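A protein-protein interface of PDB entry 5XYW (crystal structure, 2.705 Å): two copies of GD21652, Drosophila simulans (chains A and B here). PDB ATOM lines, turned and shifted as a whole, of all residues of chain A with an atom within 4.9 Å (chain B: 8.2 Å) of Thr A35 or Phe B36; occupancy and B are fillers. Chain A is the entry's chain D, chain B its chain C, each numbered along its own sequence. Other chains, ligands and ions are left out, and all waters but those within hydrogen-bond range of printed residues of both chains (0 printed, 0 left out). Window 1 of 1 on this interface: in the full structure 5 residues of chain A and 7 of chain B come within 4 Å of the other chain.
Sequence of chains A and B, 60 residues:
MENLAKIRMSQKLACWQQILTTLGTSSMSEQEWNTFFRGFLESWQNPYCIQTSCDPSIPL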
ATOM      1  N   GLN A  31      24.998  10.174  16.683  1.00  0.00           N
ATOM      2  CA  GLN A  31      24.887   8.760  17.012  1.00  0.00           C
ATOM      3  C   GLN A  31      25.969   7.938  16.291  1.00  0.00           C
ATOM      4  O   GLN A  31      26.509   6.994  16.862  1.00  0.00           O
ATOM      5  CB  GLN A  31      23.470   8.259  16.707  1.00  0.00           C
ATOM      6  CG  GLN A  31      23.280   6.762  16.828  1.00  0.00           C
ATOM      7  CD  GLN A  31      21.926   6.330  16.338  1.00  0.00           C
ATOM      8  OE1 GLN A  31      21.203   5.606  17.021  1.00  0.00           O
ATOM      9  NE2 GLN A  31      21.568   6.775  15.146  1.00  0.00           N
ATOM     10  N   GLU A  32      26.226   8.256  15.021  1.00  0.00           N
ATOM     11  CA  GLU A  32      27.333   7.630  14.302  1.00  0.00           C
ATOM     12  C   GLU A  32      28.633   7.870  15.043  1.00  0.00           C
ATOM     13  O   GLU A  32      29.357   6.927  15.360  1.00  0.00           O
ATOM     14  CB  GLU A  32      27.480   8.150  12.870  1.00  0.00           C
ATOM     15  CG  GLU A  32      26.661   7.412  11.827  1.00  0.00           C
ATOM     16  CD  GLU A  32      26.596   8.153  10.504  1.00  0.00           C
ATOM     17  OE1 GLU A  32      27.232   9.221  10.382  1.00  0.00           O
ATOM     18  OE2 GLU A  32      25.913   7.665   9.582  1.00  0.00           O
ATOM     19  N   TRP A  33      28.911   9.141  15.314  1.00  0.00           N
ATOM     20  CA  TRP A  33      30.129   9.541  16.000  1.00  0.00           C
ATOM     21  C   TRP A  33      30.297   8.727  17.274  1.00  0.00           C
ATOM     22  O   TRP A  33      31.354   8.138  17.504  1.00  0.00           O
ATOM     23  CB  TRP A  33      30.085  11.038  16.320  1.00  0.00           C
ATOM     24  CG  TRP A  33      31.399  11.650  16.657  1.00  0.00           C
ATOM     25  CD1 TRP A  33      32.203  12.358  15.819  1.00  0.00           C
ATOM     26  CD2 TRP A  33      32.063  11.631  17.929  1.00  0.00           C
ATOM     27  NE1 TRP A  33      33.333  12.774  16.483  1.00  0.00           N
ATOM     28  CE2 TRP A  33      33.272  12.338  17.779  1.00  0.00           C
ATOM     29  CE3 TRP A  33      31.755  11.076  19.175  1.00  0.00           C
ATOM     30  CZ2 TRP A  33      34.175  12.509  18.826  1.00  0.00           C
ATOM     31  CZ3 TRP A  33      32.649  11.245  20.213  1.00  0.00           C
ATOM     32  CH2 TRP A  33      33.850  11.953  20.030  1.00  0.00           C
ATOM     33  N   ASN A  34      29.246   8.660  18.087  1.00  0.00           N
ATOM     34  CA  ASN A  34      29.350   7.895  19.327  1.00  0.00           C
ATOM     35  C   ASN A  34      29.578   6.388  19.125  1.00  0.00           C
ATOM     36  O   ASN A  34      30.393   5.769  19.813  1.00  0.00           O
ATOM     37  CB  ASN A  34      28.120   8.140  20.189  1.00  0.00           C
ATOM     38  CG  ASN A  34      28.239   9.412  21.004  1.00  0.00           C
ATOM     39  OD1 ASN A  34      29.290   9.691  21.574  1.00  0.00           O
ATOM     40  ND2 ASN A  34      27.159  10.187  21.073  1.00  0.00           N
ATOM     41  N   THR A  35      28.836   5.793  18.208  1.00  0.00           N
ATOM     42  CA  THR A  35      28.936   4.360  17.964  1.00  0.00           C
ATOM     43  C   THR A  35      30.332   3.965  17.443  1.00  0.00           C
ATOM     44  O   THR A  35      30.971   3.024  17.945  1.00  0.00           O
ATOM     45  CB  THR A  35      27.796   3.933  17.000  1.00  0.00           C
ATOM     46  OG1 THR A  35      26.550   4.334  17.583  1.00  0.00           O
ATOM     47  CG2 THR A  35      27.771   2.417  16.737  1.00  0.00           C
ATOM     48  N   PHE A  36      30.792   4.710  16.446  1.00  0.00           N
ATOM     49  CA  PHE A  36      32.110   4.537  15.828  1.00  0.00           C
ATOM     50  C   PHE A  36      33.237   4.798  16.823  1.00  0.00           C
ATOM     51  O   PHE A  36      34.246   4.099  16.828  1.00  0.00           O
ATOM     52  CB  PHE A  36      32.231   5.465  14.626  1.00  0.00           C
ATOM     53  CG  PHE A  36      31.324   5.078  13.500  1.00  0.00           C
ATOM     54  CD1 PHE A  36      31.086   5.938  12.447  1.00  0.00           C
ATOM     55  CD2 PHE A  36      30.655   3.863  13.531  1.00  0.00           C
ATOM     56  CE1 PHE A  36      30.232   5.599  11.434  1.00  0.00           C
ATOM     57  CE2 PHE A  36      29.797   3.508  12.519  1.00  0.00           C
ATOM     58  CZ  PHE A  36      29.584   4.378  11.465  1.00  0.00           C
ATOM     59  N   PHE A  37      33.075   5.820  17.655  1.00  0.00           N
ATOM     60  CA  PHE A  37      34.044   6.065  18.706  1.00  0.00           C
ATOM     61  C   PHE A  37      34.106   4.942  19.746  1.00  0.00           C
ATOM     62  O   PHE A  37      35.170   4.643  20.287  1.00  0.00           O
ATOM     63  CB  PHE A  37      33.751   7.381  19.406  1.00  0.00           C
ATOM     64  CG  PHE A  37      34.603   7.600  20.615  1.00  0.00           C
ATOM     65  CD1 PHE A  37      35.970   7.812  20.496  1.00  0.00           C
ATOM     66  CD2 PHE A  37      34.037   7.540  21.883  1.00  0.00           C
ATOM     67  CE1 PHE A  37      36.747   7.979  21.619  1.00  0.00           C
ATOM     68  CE2 PHE A  37      34.805   7.708  23.003  1.00  0.00           C
ATOM     69  CZ  PHE A  37      36.156   7.924  22.871  1.00  0.00           C
ATOM     70  N   ARG A  38      32.974   4.334  20.061  1.00  0.00           N
ATOM     71  CA  ARG A  38      33.010   3.220  21.000  1.00  0.00           C
ATOM     72  C   ARG A  38      33.644   1.971  20.377  1.00  0.00           C
ATOM     73  O   ARG A  38      34.402   1.247  21.036  1.00  0.00           O
ATOM     74  CB  ARG A  38      31.605   2.920  21.511  1.00  0.00           C
ATOM     75  CG  ARG A  38      31.537   1.709  22.426  1.00  0.00           C
ATOM     76  CD  ARG A  38      30.081   1.285  22.576  1.00  0.00           C
ATOM     77  NE  ARG A  38      29.979  -0.144  22.844  1.00  0.00           N
ATOM     78  CZ  ARG A  38      29.887  -1.065  21.882  1.00  0.00           C
ATOM     79  NH1 ARG A  38      29.888  -0.709  20.594  1.00  0.00           N
ATOM     80  NH2 ARG A  38      29.786  -2.346  22.204  1.00  0.00           N
ATOM     81  N   GLY A  39      33.391   1.746  19.094  1.00  0.00           N
ATOM     82  CA  GLY A  39      34.062   0.646  18.415  1.00  0.00           C
ATOM     83  C   GLY A  39      35.559   0.938  18.355  1.00  0.00           C
ATOM     84  O   GLY A  39      36.430   0.051  18.403  1.00  0.00           O
ATOM     85  N   TRP B  16      28.848  -9.927   5.750  1.00  0.00           N
ATOM     86  CA  TRP B  16      28.229  -9.413   6.945  1.00  0.00           C
ATOM     87  C   TRP B  16      27.896 -10.547   7.906  1.00  0.00           C
ATOM     88  O   TRP B  16      28.019 -10.397   9.122  1.00  0.00           O
ATOM     89  CB  TRP B  16      26.985  -8.625   6.611  1.00  0.00           C
ATOM     90  CG  TRP B  16      26.379  -8.024   7.817  1.00  0.00           C
ATOM     91  CD1 TRP B  16      25.220  -8.388   8.429  1.00  0.00           C
ATOM     92  CD2 TRP B  16      26.899  -6.923   8.567  1.00  0.00           C
ATOM     93  NE1 TRP B  16      24.976  -7.569   9.511  1.00  0.00           N
ATOM     94  CE2 TRP B  16      25.997  -6.666   9.617  1.00  0.00           C
ATOM     95  CE3 TRP B  16      28.037  -6.121   8.437  1.00  0.00           C
ATOM     96  CZ2 TRP B  16      26.201  -5.653  10.541  1.00  0.00           C
ATOM     97  CZ3 TRP B  16      28.237  -5.113   9.355  1.00  0.00           C
ATOM     98  CH2 TRP B  16      27.328  -4.887  10.396  1.00  0.00           C
ATOM     99  N   ILE B  19      30.890 -11.511   9.598  1.00  0.00           N
ATOM    100  CA  ILE B  19      31.215 -10.497  10.583  1.00  0.00           C
ATOM    101  C   ILE B  19      30.436 -10.766  11.884  1.00  0.00           C
ATOM    102  O   ILE B  19      31.014 -10.792  12.983  1.00  0.00           O
ATOM    103  CB  ILE B  19      30.936  -9.068  10.008  1.00  0.00           C
ATOM    104  CG1 ILE B  19      32.068  -8.671   9.043  1.00  0.00           C
ATOM    105  CG2 ILE B  19      30.872  -8.009  11.099  1.00  0.00           C
ATOM    106  CD1 ILE B  19      31.883  -7.290   8.351  1.00  0.00           C
ATOM    107  N   LEU B  23      32.205 -11.525  15.561  1.00  0.00           N
ATOM    108  CA  LEU B  23      32.002 -10.694  16.748  1.00  0.00           C
ATOM    109  C   LEU B  23      30.974 -11.274  17.716  1.00  0.00           C
ATOM    110  O   LEU B  23      31.142 -11.155  18.930  1.00  0.00           O
ATOM    111  CB  LEU B  23      31.577  -9.280  16.356  1.00  0.00           C
ATOM    112  CG  LEU B  23      32.388  -8.610  15.259  1.00  0.00           C
ATOM    113  CD1 LEU B  23      31.825  -7.248  14.962  1.00  0.00           C
ATOM    114  CD2 LEU B  23      33.875  -8.540  15.645  1.00  0.00           C
ATOM    115  N   MET B  28      26.775  -6.214  20.565  1.00  0.00           N
ATOM    116  CA  MET B  28      26.283  -4.847  20.454  1.00  0.00           C
ATOM    117  C   MET B  28      24.782  -4.853  20.621  1.00  0.00           C
ATOM    118  O   MET B  28      24.133  -5.897  20.553  1.00  0.00           O
ATOM    119  CB  MET B  28      26.580  -4.201  19.091  1.00  0.00           C
ATOM    120  CG  MET B  28      27.988  -4.329  18.548  1.00  0.00           C
ATOM    121  SD  MET B  28      28.132  -3.342  17.062  1.00  0.00           S
ATOM    122  CE  MET B  28      28.602  -1.848  17.896  1.00  0.00           C
ATOM    123  N   SER B  29      24.227  -3.678  20.860  1.00  0.00           N
ATOM    124  CA  SER B  29      22.791  -3.512  20.730  1.00  0.00           C
ATOM    125  C   SER B  29      22.439  -3.494  19.246  1.00  0.00           C
ATOM    126  O   SER B  29      23.307  -3.363  18.395  1.00  0.00           O
ATOM    127  CB  SER B  29      22.325  -2.231  21.417  1.00  0.00           C
ATOM    128  OG  SER B  29      22.615  -1.095  20.629  1.00  0.00           O
ATOM    129  N   GLU B  30      21.160  -3.642  18.935  1.00  0.00           N
ATOM    130  CA  GLU B  30      20.698  -3.625  17.555  1.00  0.00           C
ATOM    131  C   GLU B  30      20.869  -2.240  16.926  1.00  0.00           C
ATOM    132  O   GLU B  30      21.061  -2.128  15.721  1.00  0.00           O
ATOM    133  CB  GLU B  30      19.244  -4.110  17.449  1.00  0.00           C
ATOM    134  CG  GLU B  30      18.223  -3.482  18.399  1.00  0.00           C
ATOM    135  CD  GLU B  30      18.285  -4.049  19.815  1.00  0.00           C
ATOM    136  OE1 GLU B  30      19.295  -4.702  20.163  1.00  0.00           O
ATOM    137  OE2 GLU B  30      17.303  -3.868  20.569  1.00  0.00           O
ATOM    138  N   GLN B  31      20.807  -1.189  17.738  1.00  0.00           N
ATOM    139  CA  GLN B  31      20.971   0.174  17.237  1.00  0.00           C
ATOM    140  C   GLN B  31      22.376   0.325  16.648  1.00  0.00           C
ATOM    141  O   GLN B  31      22.569   0.761  15.501  1.00  0.00           O
ATOM    142  CB  GLN B  31      20.787   1.170  18.388  1.00  0.00           C
ATOM    143  CG  GLN B  31      21.236   2.602  18.091  1.00  0.00           C
ATOM    144  CD  GLN B  31      21.360   3.483  19.350  1.00  0.00           C
ATOM    145  OE1 GLN B  31      21.964   3.079  20.350  1.00  0.00           O
ATOM    146  NE2 GLN B  31      20.820   4.699  19.284  1.00  0.00           N
ATOM    147  N   GLU B  32      23.331  -0.129  17.446  1.00  0.00           N
ATOM    148  CA  GLU B  32      24.737  -0.167  17.130  1.00  0.00           C
ATOM    149  C   GLU B  32      24.982  -0.967  15.859  1.00  0.00           C
ATOM    150  O   GLU B  32      25.572  -0.465  14.889  1.00  0.00           O
ATOM    151  CB  GLU B  32      25.451  -0.789  18.312  1.00  0.00           C
ATOM    152  CG  GLU B  32      25.731   0.190  19.431  1.00  0.00           C
ATOM    153  CD  GLU B  32      26.040  -0.512  20.739  1.00  0.00           C
ATOM    154  OE1 GLU B  32      25.131  -0.620  21.590  1.00  0.00           O
ATOM    155  OE2 GLU B  32      27.182  -0.967  20.919  1.00  0.00           O
ATOM    156  N   TRP B  33      24.501  -2.209  15.869  1.00  0.00           N
ATOM    157  CA  TRP B  33      24.632  -3.101  14.725  1.00  0.00           C
ATOM    158  C   TRP B  33      24.119  -2.419  13.466  1.00  0.00           C
ATOM    159  O   TRP B  33      24.713  -2.537  12.412  1.00  0.00           O
ATOM    160  CB  TRP B  33      23.894  -4.410  14.937  1.00  0.00           C
ATOM    161  CG  TRP B  33      24.652  -5.445  15.706  1.00  0.00           C
ATOM    162  CD1 TRP B  33      24.319  -5.977  16.922  1.00  0.00           C
ATOM    163  CD2 TRP B  33      25.870  -6.079  15.310  1.00  0.00           C
ATOM    164  NE1 TRP B  33      25.255  -6.914  17.304  1.00  0.00           N
ATOM    165  CE2 TRP B  33      26.224  -6.986  16.337  1.00  0.00           C
ATOM    166  CE3 TRP B  33      26.711  -5.954  14.201  1.00  0.00           C
ATOM    167  CZ2 TRP B  33      27.376  -7.767  16.278  1.00  0.00           C
ATOM    168  CZ3 TRP B  33      27.853  -6.735  14.143  1.00  0.00           C
ATOM    169  CH2 TRP B  33      28.173  -7.633  15.175  1.00  0.00           C
ATOM    170  N   ASN B  34      22.971  -1.757  13.558  1.00  0.00           N
ATOM    171  CA  ASN B  34      22.424  -1.049  12.400  1.00  0.00           C
ATOM    172  C   ASN B  34      23.314   0.075  11.903  1.00  0.00           C
ATOM    173  O   ASN B  34      23.531   0.208  10.710  1.00  0.00           O
ATOM    174  CB  ASN B  34      21.037  -0.482  12.702  1.00  0.00           C
ATOM    175  CG  ASN B  34      19.946  -1.496  12.488  1.00  0.00           C
ATOM    176  OD1 ASN B  34      19.971  -2.236  11.502  1.00  0.00           O
ATOM    177  ND2 ASN B  34      18.968  -1.526  13.390  1.00  0.00           N
ATOM    178  N   THR B  35      23.825   0.891  12.817  1.00  0.00           N
ATOM    179  CA  THR B  35      24.675   1.998  12.399  1.00  0.00           C
ATOM    180  C   THR B  35      25.905   1.481  11.642  1.00  0.00           C
ATOM    181  O   THR B  35      26.215   1.951  10.538  1.00  0.00           O
ATOM    182  CB  THR B  35      25.142   2.813  13.573  1.00  0.00           C
ATOM    183  OG1 THR B  35      24.004   3.264  14.291  1.00  0.00           O
ATOM    184  CG2 THR B  35      25.978   4.006  13.079  1.00  0.00           C
ATOM    185  N   PHE B  36      26.566   0.488  12.234  1.00  0.00           N
ATOM    186  CA  PHE B  36      27.667  -0.182  11.557  1.00  0.00           C
ATOM    187  C   PHE B  36      27.271  -0.868  10.252  1.00  0.00           C
ATOM    188  O   PHE B  36      28.031  -0.836   9.310  1.00  0.00           O
ATOM    189  CB  PHE B  36      28.342  -1.201  12.474  1.00  0.00           C
ATOM    190  CG  PHE B  36      29.322  -0.587  13.426  1.00  0.00           C
ATOM    191  CD1 PHE B  36      30.446   0.063  12.928  1.00  0.00           C
ATOM    192  CD2 PHE B  36      29.150  -0.666  14.800  1.00  0.00           C
ATOM    193  CE1 PHE B  36      31.363   0.636  13.776  1.00  0.00           C
ATOM    194  CE2 PHE B  36      30.083  -0.089  15.656  1.00  0.00           C
ATOM    195  CZ  PHE B  36      31.180   0.562  15.151  1.00  0.00           C
ATOM    196  N   PHE B  37      26.104  -1.489  10.191  1.00  0.00           N
ATOM    197  CA  PHE B  37      25.664  -2.123   8.958  1.00  0.00           C
ATOM    198  C   PHE B  37      25.445  -1.101   7.847  1.00  0.00           C
ATOM    199  O   PHE B  37      25.730  -1.359   6.672  1.00  0.00           O
ATOM    200  CB  PHE B  37      24.381  -2.910   9.182  1.00  0.00           C
ATOM    201  CG  PHE B  37      23.888  -3.608   7.962  1.00  0.00           C
ATOM    202  CD1 PHE B  37      24.583  -4.691   7.462  1.00  0.00           C
ATOM    203  CD2 PHE B  37      22.763  -3.178   7.292  1.00  0.00           C
ATOM    204  CE1 PHE B  37      24.157  -5.356   6.323  1.00  0.00           C
ATOM    205  CE2 PHE B  37      22.333  -3.835   6.148  1.00  0.00           C
ATOM    206  CZ  PHE B  37      23.035  -4.927   5.667  1.00  0.00           C
ATOM    207  N   ARG B  38      24.962   0.073   8.212  1.00  0.00           N
ATOM    208  CA  ARG B  38      24.725   1.098   7.216  1.00  0.00           C
ATOM    209  C   ARG B  38      26.110   1.587   6.753  1.00  0.00           C
ATOM    210  O   ARG B  38      26.349   1.834   5.549  1.00  0.00           O
ATOM    211  CB  ARG B  38      23.847   2.226   7.810  1.00  0.00           C
ATOM    212  CG  ARG B  38      23.396   3.304   6.805  1.00  0.00           C
ATOM    213  CD  ARG B  38      22.744   4.566   7.396  1.00  0.00           C
ATOM    214  NE  ARG B  38      22.591   5.600   6.357  1.00  0.00           N
ATOM    215  CZ  ARG B  38      23.512   6.513   6.039  1.00  0.00           C
ATOM    216  NH1 ARG B  38      24.671   6.538   6.687  1.00  0.00           N
ATOM    217  NH2 ARG B  38      23.277   7.400   5.068  1.00  0.00           N
ATOM    218  N   GLY B  39      27.058   1.642   7.691  1.00  0.00           N
ATOM    219  CA  GLY B  39      28.421   2.004   7.318  1.00  0.00           C
ATOM    220  C   GLY B  39      29.120   0.958   6.439  1.00  0.00           C
ATOM    221  O   GLY B  39      29.870   1.276   5.522  1.00  0.00           O
ATOM    222  N   PHE B  40      28.822  -0.302   6.706  1.00  0.00           N
ATOM    223  CA  PHE B  40      29.321  -1.409   5.943  1.00  0.00           C
ATOM    224  C   PHE B  40      28.833  -1.340   4.522  1.00  0.00           C
ATOM    225  O   PHE B  40      29.546  -1.722   3.602  1.00  0.00           O
ATOM    226  CB  PHE B  40      28.917  -2.723   6.588  1.00  0.00           C
ATOM    227  CG  PHE B  40      29.186  -3.933   5.721  1.00  0.00           C
ATOM    228  CD1 PHE B  40      30.464  -4.479   5.640  1.00  0.00           C
ATOM    229  CD2 PHE B  40      28.142  -4.546   5.014  1.00  0.00           C
ATOM    230  CE1 PHE B  40      30.708  -5.598   4.853  1.00  0.00           C
ATOM    231  CE2 PHE B  40      28.375  -5.662   4.245  1.00  0.00           C
ATOM    232  CZ  PHE B  40      29.669  -6.189   4.156  1.00  0.00           C
ATOM    233  N   LEU B  41      27.596  -0.905   4.336  1.00  0.00           N
ATOM    234  CA  LEU B  41      27.083  -0.792   2.971  1.00  0.00           C
ATOM    235  C   LEU B  41      27.699   0.383   2.229  1.00  0.00           C
ATOM    236  O   LEU B  41      28.153   0.232   1.087  1.00  0.00           O
ATOM    237  CB  LEU B  41      25.572  -0.668   2.977  1.00  0.00           C
ATOM    238  CG  LEU B  41      24.957  -1.984   3.432  1.00  0.00           C
ATOM    239  CD1 LEU B  41      23.466  -1.847   3.636  1.00  0.00           C
ATOM    240  CD2 LEU B  41      25.262  -3.073   2.418  1.00  0.00           C
ATOM    241  N   GLU B  42      27.743   1.550   2.863  1.00  0.00           N
ATOM    242  CA  GLU B  42      28.303   2.706   2.164  1.00  0.00           C
ATOM    243  C   GLU B  42      29.816   2.526   1.946  1.00  0.00           C
ATOM    244  O   GLU B  42      30.446   3.221   1.146  1.00  0.00           O
ATOM    245  CB  GLU B  42      28.013   3.974   2.958  1.00  0.00           C
ATOM    246  CG  GLU B  42      26.542   4.252   3.121  1.00  0.00           C
ATOM    247  CD  GLU B  42      26.246   5.419   4.047  1.00  0.00           C
ATOM    248  OE1 GLU B  42      25.338   6.211   3.711  1.00  0.00           O
ATOM    249  OE2 GLU B  42      26.906   5.539   5.107  1.00  0.00           O
ATOM    250  N   SER B  43      30.380   1.567   2.668  1.00  0.00           N
ATOM    251  CA  SER B  43      31.765   1.155   2.524  1.00  0.00           C
ATOM    252  C   SER B  43      32.172   0.720   1.114  1.00  0.00           C
ATOM    253  O   SER B  43      33.160   1.197   0.576  1.00  0.00           O
ATOM    254  CB  SER B  43      32.023   0.015   3.499  1.00  0.00           C
ATOM    255  OG  SER B  43      33.176  -0.703   3.148  1.00  0.00           O
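Hydrophobic or aromatic side chains of chain A within 4 Å of the printed part of chain B: Phe A36.
Hydrophobic or aromatic side chains of chain B that line the printed part of chain A: Met B28 and Phe B36.
Among the printed residues, Asp or Glu carboxylates within 4 Å of a Lys or Arg side-chain nitrogen of the other chain: Glu A32 with Arg B38 (3.3 Å) and Arg A38 with Glu B32 (2.7 Å).
Among the printed residues, pairs that only touch across the chains: Arg A38 with Met B28 (3.2 Å), Phe A36 with Phe B36 (3.3 Å), Thr A35 with Phe B36 (3.6 Å), Glu A32 with Thr B35 (3.7 Å) and Phe A36 with Thr B35 (3.9 Å).
Gln B31 touches its own counterpart, Gln A31.
Glu A32 touches Thr B35, but with the chains exchanged Thr A35 does not touch Glu B32 (4.005 Å).
Glu A32 touches Arg B38, and with the chains exchanged Arg A38 touches Glu B32.
Phe B36 touches its own counterpart, Phe A36.
Positions printed for both chains: 31, 32, 33, 34, 35, 36, 37, 38 and 39.
Of the 8 pairs that touch across the chains among the printed residues, 6 have their exchanged pair printed and touching as well.
The side-chain amide nitrogen (NE2) of Gln B31 is in hydrogen-bond range of the side-chain amide oxygen (OE1) of Gln A31 (2.5 Å).
The side-chain carboxylate of Glu B32 lies within salt-bridge range of the guanidinium group of Arg A38 (2.7 Å).
The guanidinium group of Arg B38 lies within salt-bridge range of the side-chain carboxylate of Glu A32 (3.3 Å).
Trp A33 touches none of the printed residues of chain B.
Of the printed residues of chain A, Gln B31 touches Gln A31 (2.5 Å).
Asn B34 touches none of the printed residues of chain A.
Of chain A, only Thr A35 (3.6 Å) and Phe A36 (3.3 Å) come within 4 Å of Phe B36.
Printed residues of chain A within 4 Å of Arg B38: Glu A32.
The nearest printed residue of chain B that does not touch Thr A35 is Glu B32 (4.005 Å).
The nearest residue of chain A that does not touch Phe B36 is Gly A39 (4.4 Å).
The side-chain hydroxyl of Ser B29 lies close to the backbone NH of Gln B31, at 3.4 Å.
The side-chain carboxylate of Glu B32 sits at hydrogen-bond distance from the side-chain hydroxyl of Ser B29, 2.7 Å away.
O of Gln B31 is in hydrogen-bond range of OG1 of Thr B35.
The guanidinium group (NH2) of Arg B38 is in salt-bridge range of the side-chain carboxylate (OE1) of Glu B42 (2.7 Å).
The side-chain hydroxyl (OG1) of Thr A35 sits at hydrogen-bond distance from the backbone carbonyl oxygen (O) of Gln A31, 2.8 Å away.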
